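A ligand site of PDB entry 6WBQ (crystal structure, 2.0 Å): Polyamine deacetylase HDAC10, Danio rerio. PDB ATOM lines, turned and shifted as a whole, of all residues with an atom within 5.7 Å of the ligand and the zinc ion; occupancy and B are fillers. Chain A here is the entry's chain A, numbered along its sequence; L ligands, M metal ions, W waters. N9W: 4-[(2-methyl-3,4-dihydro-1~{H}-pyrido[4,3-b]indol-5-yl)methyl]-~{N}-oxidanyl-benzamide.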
ATOM      1  N   ASP A  22       6.809  -9.782  -9.156  1.00  0.00           N
ATOM      2  CA  ASP A  22       7.208 -10.069  -7.786  1.00  0.00           C
ATOM      3  C   ASP A  22       7.100  -8.764  -7.024  1.00  0.00           C
ATOM      4  O   ASP A  22       8.022  -7.926  -7.100  1.00  0.00           O
ATOM      5  CB  ASP A  22       8.622 -10.646  -7.733  1.00  0.00           C
ATOM      6  CG  ASP A  22       9.005 -11.154  -6.348  1.00  0.00           C
ATOM      7  OD1 ASP A  22       8.412 -10.682  -5.344  1.00  0.00           O
ATOM      8  OD2 ASP A  22       9.900 -12.011  -6.261  1.00  0.00           O
ATOM      9  N   GLU A  24       7.594  -7.984  -4.050  1.00  0.00           N
ATOM     10  CA  GLU A  24       8.650  -7.750  -3.071  1.00  0.00           C
ATOM     11  C   GLU A  24       9.855  -7.067  -3.705  1.00  0.00           C
ATOM     12  O   GLU A  24      10.347  -6.056  -3.190  1.00  0.00           O
ATOM     13  CB  GLU A  24       9.071  -9.072  -2.435  1.00  0.00           C
ATOM     14  CG  GLU A  24       7.981  -9.814  -1.694  1.00  0.00           C
ATOM     15  CD  GLU A  24       8.160  -9.763  -0.195  1.00  0.00           C
ATOM     16  OE1 GLU A  24       8.736  -8.779   0.324  1.00  0.00           O
ATOM     17  OE2 GLU A  24       7.737 -10.736   0.465  1.00  0.00           O
ATOM     18  N   CYS A  25      10.343  -7.610  -4.829  1.00  0.00           N
ATOM     19  CA  CYS A  25      11.566  -7.106  -5.445  1.00  0.00           C
ATOM     20  C   CYS A  25      11.342  -5.923  -6.368  1.00  0.00           C
ATOM     21  O   CYS A  25      12.327  -5.320  -6.811  1.00  0.00           O
ATOM     22  CB  CYS A  25      12.254  -8.206  -6.272  1.00  0.00           C
ATOM     23  SG  CYS A  25      12.609  -9.745  -5.408  1.00  0.00           S
ATOM     24  N   ILE A  27      10.756  -2.962  -6.075  1.00  0.00           N
ATOM     25  CA  ILE A  27      11.213  -1.641  -5.676  1.00  0.00           C
ATOM     26  C   ILE A  27      12.640  -1.376  -6.105  1.00  0.00           C
ATOM     27  O   ILE A  27      13.078  -0.219  -6.070  1.00  0.00           O
ATOM     28  CB  ILE A  27      11.114  -1.430  -4.151  1.00  0.00           C
ATOM     29  CG1 ILE A  27      11.905  -2.522  -3.425  1.00  0.00           C
ATOM     30  CG2 ILE A  27       9.657  -1.427  -3.702  1.00  0.00           C
ATOM     31  CD1 ILE A  27      12.116  -2.198  -1.985  1.00  0.00           C
ATOM     32  N   ASN A  93      17.581 -16.029  -1.556  1.00  0.00           N
ATOM     33  CA  ASN A  93      16.531 -15.263  -0.890  1.00  0.00           C
ATOM     34  C   ASN A  93      16.557 -13.804  -1.319  1.00  0.00           C
ATOM     35  O   ASN A  93      17.610 -13.159  -1.272  1.00  0.00           O
ATOM     36  CB  ASN A  93      16.693 -15.389   0.633  1.00  0.00           C
ATOM     37  CG  ASN A  93      15.539 -14.760   1.393  1.00  0.00           C
ATOM     38  OD1 ASN A  93      15.748 -13.911   2.247  1.00  0.00           O
ATOM     39  ND2 ASN A  93      14.321 -15.184   1.080  1.00  0.00           N
ATOM     40  N   ALA A  94      15.394 -13.282  -1.743  1.00  0.00           N
ATOM     41  CA  ALA A  94      15.162 -11.852  -1.947  1.00  0.00           C
ATOM     42  C   ALA A  94      16.119 -11.247  -2.979  1.00  0.00           C
ATOM     43  O   ALA A  94      16.634 -10.140  -2.810  1.00  0.00           O
ATOM     44  CB  ALA A  94      15.235 -11.088  -0.617  1.00  0.00           C
ATOM     45  N   VAL A  95      16.371 -11.960  -4.059  1.00  0.00           N
ATOM     46  CA  VAL A  95      17.272 -11.465  -5.092  1.00  0.00           C
ATOM     47  C   VAL A  95      16.767 -11.954  -6.447  1.00  0.00           C
ATOM     48  O   VAL A  95      16.228 -13.055  -6.551  1.00  0.00           O
ATOM     49  CB  VAL A  95      18.728 -11.890  -4.814  1.00  0.00           C
ATOM     50  CG1 VAL A  95      18.910 -13.388  -5.005  1.00  0.00           C
ATOM     51  CG2 VAL A  95      19.700 -11.112  -5.717  1.00  0.00           C
ATOM     52  N   HIS A 136      25.670  -5.269   0.499  1.00  0.00           N
ATOM     53  CA  HIS A 136      26.028  -5.647   1.869  1.00  0.00           C
ATOM     54  C   HIS A 136      25.355  -6.932   2.367  1.00  0.00           C
ATOM     55  O   HIS A 136      25.840  -7.517   3.346  1.00  0.00           O
ATOM     56  CB  HIS A 136      25.791  -4.464   2.853  1.00  0.00           C
ATOM     57  CG  HIS A 136      24.358  -4.044   3.022  1.00  0.00           C
ATOM     58  ND1 HIS A 136      23.904  -3.416   4.156  1.00  0.00           N
ATOM     59  CD2 HIS A 136      23.285  -4.127   2.194  1.00  0.00           C
ATOM     60  CE1 HIS A 136      22.632  -3.130   4.033  1.00  0.00           C
ATOM     61  NE2 HIS A 136      22.231  -3.545   2.840  1.00  0.00           N
ATOM     62  N   HIS A 137      24.325  -7.422   1.689  1.00  0.00           N
ATOM     63  CA  HIS A 137      23.729  -8.717   2.020  1.00  0.00           C
ATOM     64  C   HIS A 137      24.423  -9.918   1.379  1.00  0.00           C
ATOM     65  O   HIS A 137      24.228 -11.037   1.849  1.00  0.00           O
ATOM     66  CB  HIS A 137      22.255  -8.778   1.610  1.00  0.00           C
ATOM     67  CG  HIS A 137      21.394  -7.789   2.330  1.00  0.00           C
ATOM     68  ND1 HIS A 137      21.434  -7.617   3.695  1.00  0.00           N
ATOM     69  CD2 HIS A 137      20.492  -6.888   1.862  1.00  0.00           C
ATOM     70  CE1 HIS A 137      20.583  -6.657   4.040  1.00  0.00           C
ATOM     71  NE2 HIS A 137      20.005  -6.205   2.938  1.00  0.00           N
ATOM     72  N   GLY A 145      19.174 -10.520  -0.954  1.00  0.00           N
ATOM     73  CA  GLY A 145      18.650  -9.185  -0.734  1.00  0.00           C
ATOM     74  C   GLY A 145      19.077  -8.169  -1.797  1.00  0.00           C
ATOM     75  O   GLY A 145      19.636  -7.128  -1.450  1.00  0.00           O
ATOM     76  N   PHE A 146      18.841  -8.476  -3.076  1.00  0.00           N
ATOM     77  CA  PHE A 146      19.231  -7.675  -4.242  1.00  0.00           C
ATOM     78  C   PHE A 146      20.743  -7.612  -4.462  1.00  0.00           C
ATOM     79  O   PHE A 146      21.162  -7.020  -5.463  1.00  0.00           O
ATOM     80  CB  PHE A 146      18.727  -6.221  -4.179  1.00  0.00           C
ATOM     81  CG  PHE A 146      17.255  -6.091  -4.044  1.00  0.00           C
ATOM     82  CD1 PHE A 146      16.407  -6.981  -4.683  1.00  0.00           C
ATOM     83  CD2 PHE A 146      16.708  -5.090  -3.263  1.00  0.00           C
ATOM     84  CE1 PHE A 146      15.045  -6.863  -4.545  1.00  0.00           C
ATOM     85  CE2 PHE A 146      15.365  -4.968  -3.148  1.00  0.00           C
ATOM     86  CZ  PHE A 146      14.527  -5.853  -3.788  1.00  0.00           C
ATOM     87  N   CYS A 147      21.567  -8.182  -3.579  1.00  0.00           N
ATOM     88  CA  CYS A 147      23.019  -8.105  -3.706  1.00  0.00           C
ATOM     89  C   CYS A 147      23.609  -9.364  -4.332  1.00  0.00           C
ATOM     90  O   CYS A 147      23.257 -10.496  -3.955  1.00  0.00           O
ATOM     91  CB  CYS A 147      23.675  -7.852  -2.340  1.00  0.00           C
ATOM     92  SG  CYS A 147      22.914  -6.523  -1.422  1.00  0.00           S
ATOM     93  N   ASP A 174      22.418   1.894   6.094  1.00  0.00           N
ATOM     94  CA  ASP A 174      21.271   1.305   5.425  1.00  0.00           C
ATOM     95  C   ASP A 174      20.308   0.845   6.514  1.00  0.00           C
ATOM     96  O   ASP A 174      20.734   0.616   7.654  1.00  0.00           O
ATOM     97  CB  ASP A 174      21.715   0.126   4.536  1.00  0.00           C
ATOM     98  CG  ASP A 174      20.625  -0.399   3.634  1.00  0.00           C
ATOM     99  OD1 ASP A 174      20.594  -0.042   2.440  1.00  0.00           O
ATOM    100  OD2 ASP A 174      19.794  -1.224   4.089  1.00  0.00           O
ATOM    101  N   VAL A 175      19.018   0.723   6.181  1.00  0.00           N
ATOM    102  CA  VAL A 175      18.054   0.345   7.212  1.00  0.00           C
ATOM    103  C   VAL A 175      17.996  -1.158   7.423  1.00  0.00           C
ATOM    104  O   VAL A 175      17.355  -1.615   8.386  1.00  0.00           O
ATOM    105  CB  VAL A 175      16.659   0.924   6.860  1.00  0.00           C
ATOM    106  CG1 VAL A 175      15.915   0.005   5.905  1.00  0.00           C
ATOM    107  CG2 VAL A 175      15.855   1.224   8.160  1.00  0.00           C
ATOM    108  N   HIS A 176      18.637  -1.941   6.565  1.00  0.00           N
ATOM    109  CA  HIS A 176      18.725  -3.384   6.704  1.00  0.00           C
ATOM    110  C   HIS A 176      20.079  -3.762   7.280  1.00  0.00           C
ATOM    111  O   HIS A 176      21.074  -3.048   7.111  1.00  0.00           O
ATOM    112  CB  HIS A 176      18.533  -4.077   5.342  1.00  0.00           C
ATOM    113  CG  HIS A 176      17.176  -3.844   4.741  1.00  0.00           C
ATOM    114  ND1 HIS A 176      16.901  -2.791   3.905  1.00  0.00           N
ATOM    115  CD2 HIS A 176      16.018  -4.532   4.876  1.00  0.00           C
ATOM    116  CE1 HIS A 176      15.642  -2.848   3.517  1.00  0.00           C
ATOM    117  NE2 HIS A 176      15.084  -3.896   4.101  1.00  0.00           N
ATOM    118  N   PHE A 204      11.715  -8.529  11.505  1.00  0.00           N
ATOM    119  CA  PHE A 204      11.940  -7.876  10.214  1.00  0.00           C
ATOM    120  C   PHE A 204      13.078  -8.560   9.457  1.00  0.00           C
ATOM    121  O   PHE A 204      14.108  -8.903  10.043  1.00  0.00           O
ATOM    122  CB  PHE A 204      12.232  -6.374  10.370  1.00  0.00           C
ATOM    123  CG  PHE A 204      12.105  -5.615   9.074  1.00  0.00           C
ATOM    124  CD1 PHE A 204      10.883  -5.532   8.428  1.00  0.00           C
ATOM    125  CD2 PHE A 204      13.224  -5.022   8.488  1.00  0.00           C
ATOM    126  CE1 PHE A 204      10.760  -4.859   7.209  1.00  0.00           C
ATOM    127  CE2 PHE A 204      13.106  -4.336   7.270  1.00  0.00           C
ATOM    128  CZ  PHE A 204      11.863  -4.255   6.637  1.00  0.00           C
ATOM    129  N   TRP A 205      12.860  -8.774   8.160  1.00  0.00           N
ATOM    130  CA  TRP A 205      13.866  -9.349   7.287  1.00  0.00           C
ATOM    131  C   TRP A 205      15.222  -8.682   7.520  1.00  0.00           C
ATOM    132  O   TRP A 205      15.286  -7.452   7.681  1.00  0.00           O
ATOM    133  CB  TRP A 205      13.423  -9.202   5.827  1.00  0.00           C
ATOM    134  CG  TRP A 205      14.251  -9.980   4.882  1.00  0.00           C
ATOM    135  CD1 TRP A 205      14.000 -11.247   4.422  1.00  0.00           C
ATOM    136  CD2 TRP A 205      15.489  -9.566   4.289  1.00  0.00           C
ATOM    137  NE1 TRP A 205      15.014 -11.643   3.589  1.00  0.00           N
ATOM    138  CE2 TRP A 205      15.950 -10.644   3.497  1.00  0.00           C
ATOM    139  CE3 TRP A 205      16.251  -8.398   4.363  1.00  0.00           C
ATOM    140  CZ2 TRP A 205      17.132 -10.583   2.760  1.00  0.00           C
ATOM    141  CZ3 TRP A 205      17.455  -8.336   3.623  1.00  0.00           C
ATOM    142  CH2 TRP A 205      17.877  -9.424   2.835  1.00  0.00           C
ATOM    143  N   GLY A 265      23.023   3.111   2.655  1.00  0.00           N
ATOM    144  CA  GLY A 265      21.672   2.881   2.209  1.00  0.00           C
ATOM    145  C   GLY A 265      20.800   4.003   2.738  1.00  0.00           C
ATOM    146  O   GLY A 265      20.868   4.339   3.923  1.00  0.00           O
ATOM    147  N   ASP A 267      17.520   3.891   2.488  1.00  0.00           N
ATOM    148  CA  ASP A 267      16.223   3.404   2.923  1.00  0.00           C
ATOM    149  C   ASP A 267      15.998   3.614   4.414  1.00  0.00           C
ATOM    150  O   ASP A 267      14.942   3.235   4.925  1.00  0.00           O
ATOM    151  CB  ASP A 267      16.055   1.928   2.549  1.00  0.00           C
ATOM    152  CG  ASP A 267      17.240   1.067   2.943  1.00  0.00           C
ATOM    153  OD1 ASP A 267      18.100   1.482   3.755  1.00  0.00           O
ATOM    154  OD2 ASP A 267      17.289  -0.065   2.435  1.00  0.00           O
ATOM    155  N   GLU A 274      10.587   0.467   2.690  1.00  0.00           N
ATOM    156  CA  GLU A 274      11.178  -0.632   3.443  1.00  0.00           C
ATOM    157  C   GLU A 274      11.483  -0.248   4.890  1.00  0.00           C
ATOM    158  O   GLU A 274      11.181  -1.003   5.816  1.00  0.00           O
ATOM    159  CB  GLU A 274      12.462  -1.118   2.751  1.00  0.00           C
ATOM    160  CG  GLU A 274      12.184  -2.055   1.594  1.00  0.00           C
ATOM    161  CD  GLU A 274      11.806  -3.446   2.073  1.00  0.00           C
ATOM    162  OE1 GLU A 274      12.361  -3.882   3.109  1.00  0.00           O
ATOM    163  OE2 GLU A 274      10.953  -4.093   1.425  1.00  0.00           O
ATOM    164  N   GLU A 304      24.088   1.692  -1.066  1.00  0.00           N
ATOM    165  CA  GLU A 304      23.422   0.408  -0.886  1.00  0.00           C
ATOM    166  C   GLU A 304      21.988   0.565  -1.346  1.00  0.00           C
ATOM    167  O   GLU A 304      21.732   0.637  -2.568  1.00  0.00           O
ATOM    168  CB  GLU A 304      23.565  -0.092   0.565  1.00  0.00           C
ATOM    169  CG  GLU A 304      25.002  -0.294   1.027  1.00  0.00           C
ATOM    170  CD  GLU A 304      25.645  -1.600   0.518  1.00  0.00           C
ATOM    171  OE1 GLU A 304      25.017  -2.340  -0.259  1.00  0.00           O
ATOM    172  OE2 GLU A 304      26.785  -1.893   0.904  1.00  0.00           O
ATOM    173  N   GLY A 305      21.004   0.635  -0.440  1.00  0.00           N
ATOM    174  CA  GLY A 305      19.613   0.760  -0.819  1.00  0.00           C
ATOM    175  C   GLY A 305      19.076   2.191  -0.734  1.00  0.00           C
ATOM    176  O   GLY A 305      19.815   3.171  -0.648  1.00  0.00           O
ATOM    177  N   GLY A 306      17.743   2.283  -0.758  1.00  0.00           N
ATOM    178  CA  GLY A 306      17.031   3.559  -0.840  1.00  0.00           C
ATOM    179  C   GLY A 306      16.029   3.508  -1.979  1.00  0.00           C
ATOM    180  O   GLY A 306      16.419   3.398  -3.148  1.00  0.00           O
ATOM    181  N   TYR A 307      14.737   3.551  -1.669  1.00  0.00           N
ATOM    182  CA  TYR A 307      13.717   3.185  -2.645  1.00  0.00           C
ATOM    183  C   TYR A 307      12.637   4.228  -2.848  1.00  0.00           C
ATOM    184  O   TYR A 307      11.846   4.075  -3.779  1.00  0.00           O
ATOM    185  CB  TYR A 307      13.073   1.838  -2.254  1.00  0.00           C
ATOM    186  CG  TYR A 307      14.142   0.814  -2.056  1.00  0.00           C
ATOM    187  CD1 TYR A 307      14.764   0.217  -3.147  1.00  0.00           C
ATOM    188  CD2 TYR A 307      14.620   0.522  -0.780  1.00  0.00           C
ATOM    189  CE1 TYR A 307      15.784  -0.675  -2.981  1.00  0.00           C
ATOM    190  CE2 TYR A 307      15.646  -0.358  -0.603  1.00  0.00           C
ATOM    191  CZ  TYR A 307      16.226  -0.964  -1.699  1.00  0.00           C
ATOM    192  OH  TYR A 307      17.255  -1.851  -1.534  1.00  0.00           O
HETATM  193  O2  N9W L   1      17.728  -2.332   0.878  1.00  0.00           O
HETATM  194  C1  N9W L   1      17.765  -3.530   1.036  1.00  0.00           C
HETATM  195  N1  N9W L   1      18.912  -4.122   1.758  1.00  0.00           N
HETATM  196  O1  N9W L   1      19.874  -3.193   2.153  1.00  0.00           O
HETATM  197  C2  N9W L   1      16.650  -4.455   0.582  1.00  0.00           C
HETATM  198  C7  N9W L   1      16.827  -5.829   0.485  1.00  0.00           C
HETATM  199  C6  N9W L   1      15.800  -6.680   0.103  1.00  0.00           C
HETATM  200  C5  N9W L   1      14.528  -6.220  -0.205  1.00  0.00           C
HETATM  201  C4  N9W L   1      14.338  -4.842  -0.106  1.00  0.00           C
HETATM  202  C3  N9W L   1      15.369  -3.978   0.278  1.00  0.00           C
HETATM  203  C8  N9W L   1      13.424  -7.168  -0.685  1.00  0.00           C
HETATM  204  N2  N9W L   1      12.720  -8.131   0.179  1.00  0.00           N
HETATM  205  C20 N9W L   1      12.392  -7.973   1.522  1.00  0.00           C
HETATM  206  C19 N9W L   1      12.678  -6.801   2.400  1.00  0.00           C
HETATM  207  C18 N9W L   1      11.988  -6.793   3.767  1.00  0.00           C
HETATM  208  N3  N9W L   1      10.814  -7.590   3.752  1.00  0.00           N
HETATM  209  C17 N9W L   1       9.774  -6.892   2.870  1.00  0.00           C
HETATM  210  C16 N9W L   1      11.215  -9.093   3.336  1.00  0.00           C
HETATM  211  C15 N9W L   1      11.722  -9.078   1.957  1.00  0.00           C
HETATM  212  C14 N9W L   1      11.587 -10.021   0.893  1.00  0.00           C
HETATM  213  C9  N9W L   1      12.220  -9.415  -0.228  1.00  0.00           C
HETATM  214  C13 N9W L   1      11.005 -11.298   0.754  1.00  0.00           C
HETATM  215  C12 N9W L   1      11.061 -11.954  -0.462  1.00  0.00           C
HETATM  216  C11 N9W L   1      11.697 -11.350  -1.563  1.00  0.00           C
HETATM  217  C10 N9W L   1      12.251 -10.089  -1.465  1.00  0.00           C
HETATM  218 ZN    ZN M   1      18.478  -1.724   2.742  1.00  0.00          ZN
HETATM  219  O   HOH W   1      10.173  -8.553   6.923  1.00  0.00           O
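An oxygen (O2) of the ligand lies close to the side-chain hydroxyl (OH) of Tyr 307 (2.5 Å). NE2 of His 136 lies close to O1 of the ligand, 2.5 Å away. NE2 of His 137 lies within hydrogen-bond range of N1 of the ligand.
OD1 of Asn 93 is in hydrogen-bond range of NE1 of Trp 205, at 2.7 Å. The side-chain carboxylate (OD2) of Asp 22 lies within hydrogen-bond range of the side-chain sulfur (SG) of Cys 25. The side-chain carboxylate (OE1) of Glu 304 is in hydrogen-bond range of the backbone NH (N) of His 136 (3.1 Å). The backbone NH of Phe 146 sits at hydrogen-bond distance from the backbone carbonyl oxygen of Ala 94. O of Ala 94 sits close to N of Gly 145, at 3.2 Å. The side-chain sulfur (SG) of Cys 147 sits at hydrogen-bond distance from the backbone NH (N) of His 137 (3.5 Å). The side-chain carboxylate of Asp 22 is in hydrogen-bond range of the backbone NH of Glu 24, at 3.1 Å. The side-chain carboxylate (OD1) of Asp 267 sits at hydrogen-bond distance from the backbone NH (N) of Val 175 (2.7 Å).
Glu 24 touches the ligand (OE1 to C14, 3.2 Å). Cys 25 touches the ligand. Ile 27 touches the ligand (CD1 to C4, 3.9 Å). Ala 94 touches the ligand (CB to C10, 3.3 Å). O of Gly 145 touches C7 of the ligand, 3.6 Å away. Phe 146 touches the ligand. Phe 204 touches the ligand (CZ to C18, 3.8 Å). Trp 205 touches the ligand (CB to C16, 3.3 Å). OE1 of Glu 274 touches C18 of the ligand (3.0 Å). Gly 305 touches the ligand. Hydrophobic or aromatic side chains within 4 Å of the ligand: Ile 27, Ala 94, His 136, His 137, Phe 146, His 176, Phe 204, Trp 205 and Tyr 307. Within 4 Å of the ligand: Glu 24, Cys 25, Ile 27, Ala 94, His 136, His 137, Gly 145, Phe 146, Asp 174, His 176, Phe 204, Trp 205, Asp 267, Glu 274, Gly 305 and Tyr 307.
Of the 24 residues printed, 3 come within 4 Å of the zinc ion. Along chain A the residues within 4 Å of the zinc ion span positions 174 to 267. The nearest printed residue that does not touch the zinc ion is His 136 (4.2 Å).
The zinc ion is bound by OD2 of Asp 174 (1.9 Å), OD2 of Asp 267 (2.1 Å), O2 of the ligand (2.1 Å), O1 of the ligand (2.1 Å) and ND1 of His 176 (2.2 Å). The zinc ion has five donor atoms within binding distance. Slightly farther from the zinc ion lies OD1 of Asp 174 (2.7 Å).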
